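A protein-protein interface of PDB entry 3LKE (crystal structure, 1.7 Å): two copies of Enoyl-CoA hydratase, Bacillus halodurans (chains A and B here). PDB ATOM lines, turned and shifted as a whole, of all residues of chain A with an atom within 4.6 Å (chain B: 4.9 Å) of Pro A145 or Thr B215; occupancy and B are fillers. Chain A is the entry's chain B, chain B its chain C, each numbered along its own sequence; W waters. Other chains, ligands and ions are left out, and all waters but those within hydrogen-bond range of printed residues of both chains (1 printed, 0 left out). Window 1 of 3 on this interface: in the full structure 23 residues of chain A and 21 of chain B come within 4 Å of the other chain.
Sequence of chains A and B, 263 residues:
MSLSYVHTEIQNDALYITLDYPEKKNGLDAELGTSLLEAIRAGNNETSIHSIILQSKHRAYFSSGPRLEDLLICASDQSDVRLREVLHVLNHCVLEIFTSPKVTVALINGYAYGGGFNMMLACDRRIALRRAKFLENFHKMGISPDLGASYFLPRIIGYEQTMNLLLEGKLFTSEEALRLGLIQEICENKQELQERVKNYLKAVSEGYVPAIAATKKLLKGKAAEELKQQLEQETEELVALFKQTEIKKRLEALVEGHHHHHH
No position is printed for both chains.
The backbone carbonyl oxygen (O) of Ala B211 lies within hydrogen-bond range of the side-chain hydroxyl (OG1) of Thr B215 (2.7 Å).
The backbone carbonyl oxygen (O) of Phe A138 lies within hydrogen-bond range of the backbone NH (N) of Ile A143, at 3.1 Å.
N of Ala A149 is in hydrogen-bond range of OE2 of Glu A234, at 3.4 Å.
OE2 of Glu A234 sits at hydrogen-bond distance from OG of Ser A150 (2.5 Å).
Among the printed residues, pairs that only touch across the chains: Ile A143 with Ala B211 (3.9 Å), Ile A143 with Thr B215 (3.99 Å), Ser A144 with Thr B215 (3.6 Å), Ser A144 with Leu B218 (3.9 Å), Pro A145 with Thr B215 (3.4 Å), Pro A145 with Leu B218 (3.8 Å), Ser A150 with Leu B218 (3.7 Å), Ser A150 with Leu B219 (3.6 Å) and Glu A234 with Leu B218 (3.6 Å).
Water W1 lies within hydrogen-bond range of O of Ser A150 (2.7 Å) and O of Leu B219 (2.8 Å).
Printed residues of chain B within 4 Å of Ile A143: Ala B211 (3.9 Å) and Thr B215 (3.99 Å).
Printed residues of chain B within 4 Å of Ser A144: Thr B215 and Leu B218.
Of the printed residues of chain B, Pro A145 touches Thr B215 and Leu B218.
Of the printed residues of chain A, Thr B215 touches Ile A143 (3.99 Å), Ser A144 (3.6 Å) and Pro A145 (3.4 Å).
Of the printed residues of chain A, Leu B218 touches Ser A144 (3.9 Å), Pro A145 (3.8 Å), Ser A150 (3.7 Å) and Glu A234 (3.6 Å).
Of the 9 printed residues of chain B, 4 touch a printed residue of chain A.
Printed residues of chain B that touch a printed residue of chain A: Ala B211, Thr B215, Leu B218 and Leu B219.
Hydrophobic or aromatic side chains of chain B that line the printed part of chain A: Ala B211, Leu B218 and Leu B219.
Among the printed residues, no Asp or Glu carboxylate lies within 4 Å of a Lys or Arg side-chain nitrogen of the other chain.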
ATOM      1  N   PHE A 138       4.099  -2.740   8.932  1.00  0.00           N
ATOM      2  CA  PHE A 138       4.323  -3.637   7.802  1.00  0.00           C
ATOM      3  C   PHE A 138       4.677  -5.059   8.233  1.00  0.00           C
ATOM      4  O   PHE A 138       4.222  -6.037   7.630  1.00  0.00           O
ATOM      5  CB  PHE A 138       5.424  -3.088   6.875  1.00  0.00           C
ATOM      6  CG  PHE A 138       5.203  -1.662   6.430  1.00  0.00           C
ATOM      7  CD1 PHE A 138       4.310  -1.370   5.403  1.00  0.00           C
ATOM      8  CD2 PHE A 138       5.878  -0.622   7.029  1.00  0.00           C
ATOM      9  CE1 PHE A 138       4.097  -0.069   4.990  1.00  0.00           C
ATOM     10  CE2 PHE A 138       5.684   0.696   6.614  1.00  0.00           C
ATOM     11  CZ  PHE A 138       4.790   0.976   5.592  1.00  0.00           C
ATOM     12  N   ILE A 143       3.886  -7.466   4.843  1.00  0.00           N
ATOM     13  CA  ILE A 143       4.152  -6.723   3.607  1.00  0.00           C
ATOM     14  C   ILE A 143       5.430  -5.892   3.682  1.00  0.00           C
ATOM     15  O   ILE A 143       6.023  -5.715   4.749  1.00  0.00           O
ATOM     16  CB  ILE A 143       2.974  -5.805   3.211  1.00  0.00           C
ATOM     17  CG1 ILE A 143       2.802  -4.685   4.235  1.00  0.00           C
ATOM     18  CG2 ILE A 143       1.678  -6.631   3.046  1.00  0.00           C
ATOM     19  CD1 ILE A 143       1.743  -3.659   3.861  1.00  0.00           C
ATOM     20  N   SER A 144       5.868  -5.419   2.524  1.00  0.00           N
ATOM     21  CA  SER A 144       7.059  -4.596   2.423  1.00  0.00           C
ATOM     22  C   SER A 144       6.679  -3.120   2.532  1.00  0.00           C
ATOM     23  O   SER A 144       5.535  -2.751   2.306  1.00  0.00           O
ATOM     24  CB  SER A 144       7.763  -4.877   1.090  1.00  0.00           C
ATOM     25  OG  SER A 144       6.823  -4.889   0.019  1.00  0.00           O
ATOM     26  N   PRO A 145       7.643  -2.258   2.892  1.00  0.00           N
ATOM     27  CA  PRO A 145       7.311  -0.834   3.053  1.00  0.00           C
ATOM     28  C   PRO A 145       6.994  -0.193   1.703  1.00  0.00           C
ATOM     29  O   PRO A 145       7.615  -0.567   0.716  1.00  0.00           O
ATOM     30  CB  PRO A 145       8.613  -0.224   3.607  1.00  0.00           C
ATOM     31  CG  PRO A 145       9.420  -1.361   4.082  1.00  0.00           C
ATOM     32  CD  PRO A 145       9.035  -2.556   3.257  1.00  0.00           C
ATOM     33  N   ASP A 146       6.040   0.734   1.670  1.00  0.00           N
ATOM     34  CA  ASP A 146       5.675   1.424   0.437  1.00  0.00           C
ATOM     35  C   ASP A 146       5.509   2.930   0.631  1.00  0.00           C
ATOM     36  O   ASP A 146       5.853   3.483   1.675  1.00  0.00           O
ATOM     37  CB  ASP A 146       4.403   0.812  -0.178  1.00  0.00           C
ATOM     38  CG  ASP A 146       3.172   1.066   0.663  1.00  0.00           C
ATOM     39  OD1 ASP A 146       3.327   1.556   1.805  1.00  0.00           O
ATOM     40  OD2 ASP A 146       2.043   0.762   0.194  1.00  0.00           O
ATOM     41  N   ALA A 149       8.532   4.705   1.865  1.00  0.00           N
ATOM     42  CA  ALA A 149       9.055   4.431   3.210  1.00  0.00           C
ATOM     43  C   ALA A 149      10.420   3.754   3.170  1.00  0.00           C
ATOM     44  O   ALA A 149      11.271   4.007   4.042  1.00  0.00           O
ATOM     45  CB  ALA A 149       8.059   3.613   4.043  1.00  0.00           C
ATOM     46  N   SER A 150      10.632   2.894   2.173  1.00  0.00           N
ATOM     47  CA  SER A 150      11.910   2.198   2.070  1.00  0.00           C
ATOM     48  C   SER A 150      13.037   3.130   1.657  1.00  0.00           C
ATOM     49  O   SER A 150      14.199   2.811   1.883  1.00  0.00           O
ATOM     50  CB  SER A 150      11.849   0.992   1.132  1.00  0.00           C
ATOM     51  OG  SER A 150      11.790   1.389  -0.219  1.00  0.00           O
ATOM     52  N   LEU A 166      10.704  -1.268  12.402  1.00  0.00           N
ATOM     53  CA  LEU A 166       9.747  -2.104  11.692  1.00  0.00           C
ATOM     54  C   LEU A 166       9.510  -3.392  12.464  1.00  0.00           C
ATOM     55  O   LEU A 166       8.380  -3.883  12.545  1.00  0.00           O
ATOM     56  CB  LEU A 166      10.247  -2.401  10.275  1.00  0.00           C
ATOM     57  CG  LEU A 166      10.364  -1.176   9.368  1.00  0.00           C
ATOM     58  CD1 LEU A 166      11.032  -1.552   8.050  1.00  0.00           C
ATOM     59  CD2 LEU A 166       8.996  -0.545   9.129  1.00  0.00           C
ATOM     60  N   GLU A 234       9.297  -0.485  -4.999  1.00  0.00           N
ATOM     61  CA  GLU A 234       8.356  -0.781  -3.911  1.00  0.00           C
ATOM     62  C   GLU A 234       7.063  -1.331  -4.480  1.00  0.00           C
ATOM     63  O   GLU A 234       6.493  -2.276  -3.939  1.00  0.00           O
ATOM     64  CB  GLU A 234       8.019   0.457  -3.099  1.00  0.00           C
ATOM     65  CG  GLU A 234       9.158   0.925  -2.197  1.00  0.00           C
ATOM     66  CD  GLU A 234       8.826   2.219  -1.488  1.00  0.00           C
ATOM     67  OE1 GLU A 234       7.783   2.822  -1.817  1.00  0.00           O
ATOM     68  OE2 GLU A 234       9.602   2.630  -0.601  1.00  0.00           O
ATOM     69  N   ALA B 211       8.414 -11.359   2.963  1.00  0.00           N
ATOM     70  CA  ALA B 211       8.231  -9.927   3.184  1.00  0.00           C
ATOM     71  C   ALA B 211       9.458  -9.285   3.849  1.00  0.00           C
ATOM     72  O   ALA B 211       9.825  -8.149   3.518  1.00  0.00           O
ATOM     73  CB  ALA B 211       6.980  -9.660   4.016  1.00  0.00           C
ATOM     74  N   ILE B 212      10.065 -10.007   4.789  1.00  0.00           N
ATOM     75  CA  ILE B 212      11.323  -9.591   5.420  1.00  0.00           C
ATOM     76  C   ILE B 212      12.402  -9.457   4.342  1.00  0.00           C
ATOM     77  O   ILE B 212      13.145  -8.472   4.301  1.00  0.00           O
ATOM     78  CB  ILE B 212      11.769 -10.613   6.475  1.00  0.00           C
ATOM     79  CG1 ILE B 212      10.815 -10.569   7.678  1.00  0.00           C
ATOM     80  CG2 ILE B 212      13.205 -10.379   6.913  1.00  0.00           C
ATOM     81  CD1 ILE B 212      10.931 -11.781   8.611  1.00  0.00           C
ATOM     82  N   ALA B 213      12.472 -10.456   3.471  1.00  0.00           N
ATOM     83  CA  ALA B 213      13.467 -10.462   2.402  1.00  0.00           C
ATOM     84  C   ALA B 213      13.249  -9.287   1.448  1.00  0.00           C
ATOM     85  O   ALA B 213      14.212  -8.598   1.068  1.00  0.00           O
ATOM     86  CB  ALA B 213      13.431 -11.805   1.655  1.00  0.00           C
ATOM     87  N   ALA B 214      11.995  -9.031   1.084  1.00  0.00           N
ATOM     88  CA  ALA B 214      11.684  -7.948   0.157  1.00  0.00           C
ATOM     89  C   ALA B 214      11.967  -6.616   0.832  1.00  0.00           C
ATOM     90  O   ALA B 214      12.430  -5.672   0.201  1.00  0.00           O
ATOM     91  CB  ALA B 214      10.219  -8.024  -0.293  1.00  0.00           C
ATOM     92  N   THR B 215      11.697  -6.553   2.132  1.00  0.00           N
ATOM     93  CA  THR B 215      11.921  -5.322   2.874  1.00  0.00           C
ATOM     94  C   THR B 215      13.406  -4.959   2.865  1.00  0.00           C
ATOM     95  O   THR B 215      13.781  -3.801   2.589  1.00  0.00           O
ATOM     96  CB  THR B 215      11.415  -5.456   4.333  1.00  0.00           C
ATOM     97  OG1 THR B 215       9.986  -5.603   4.324  1.00  0.00           O
ATOM     98  CG2 THR B 215      11.807  -4.211   5.131  1.00  0.00           C
ATOM     99  N   LYS B 216      14.244  -5.947   3.156  1.00  0.00           N
ATOM    100  CA  LYS B 216      15.697  -5.741   3.190  1.00  0.00           C
ATOM    101  C   LYS B 216      16.229  -5.350   1.809  1.00  0.00           C
ATOM    102  O   LYS B 216      17.062  -4.459   1.674  1.00  0.00           O
ATOM    103  CB  LYS B 216      16.400  -6.996   3.689  1.00  0.00           C
ATOM    104  CG  LYS B 216      16.191  -7.231   5.177  1.00  0.00           C
ATOM    105  CD  LYS B 216      17.066  -8.361   5.688  1.00  0.00           C
ATOM    106  CE  LYS B 216      18.547  -8.072   5.490  1.00  0.00           C
ATOM    107  NZ  LYS B 216      19.309  -9.089   6.246  1.00  0.00           N
ATOM    108  N   LYS B 217      15.714  -6.018   0.780  1.00  0.00           N
ATOM    109  CA  LYS B 217      16.103  -5.711  -0.597  1.00  0.00           C
ATOM    110  C   LYS B 217      15.785  -4.253  -0.951  1.00  0.00           C
ATOM    111  O   LYS B 217      16.637  -3.556  -1.501  1.00  0.00           O
ATOM    112  CB  LYS B 217      15.394  -6.688  -1.552  1.00  0.00           C
ATOM    113  CG  LYS B 217      15.659  -6.472  -3.042  1.00  0.00           C
ATOM    114  CD  LYS B 217      14.844  -7.495  -3.858  1.00  0.00           C
ATOM    115  CE  LYS B 217      15.002  -7.314  -5.370  1.00  0.00           C
ATOM    116  NZ  LYS B 217      13.953  -8.094  -6.112  1.00  0.00           N
ATOM    117  N   LEU B 218      14.571  -3.794  -0.627  1.00  0.00           N
ATOM    118  CA  LEU B 218      14.185  -2.406  -0.867  1.00  0.00           C
ATOM    119  C   LEU B 218      15.037  -1.404  -0.090  1.00  0.00           C
ATOM    120  O   LEU B 218      15.530  -0.420  -0.649  1.00  0.00           O
ATOM    121  CB  LEU B 218      12.719  -2.187  -0.516  1.00  0.00           C
ATOM    122  CG  LEU B 218      11.718  -2.786  -1.515  1.00  0.00           C
ATOM    123  CD1 LEU B 218      10.331  -2.731  -0.933  1.00  0.00           C
ATOM    124  CD2 LEU B 218      11.762  -2.008  -2.836  1.00  0.00           C
ATOM    125  N   LEU B 219      15.184  -1.638   1.208  1.00  0.00           N
ATOM    126  CA  LEU B 219      15.959  -0.707   2.043  1.00  0.00           C
ATOM    127  C   LEU B 219      17.399  -0.554   1.536  1.00  0.00           C
ATOM    128  O   LEU B 219      17.990   0.530   1.590  1.00  0.00           O
ATOM    129  CB  LEU B 219      15.974  -1.191   3.501  1.00  0.00           C
ATOM    130  CG  LEU B 219      14.647  -1.162   4.258  1.00  0.00           C
ATOM    131  CD1 LEU B 219      14.749  -1.894   5.613  1.00  0.00           C
ATOM    132  CD2 LEU B 219      14.159   0.268   4.437  1.00  0.00           C
HETATM  133  O   HOH W   1      16.734   2.923   0.843  1.00  0.00           O
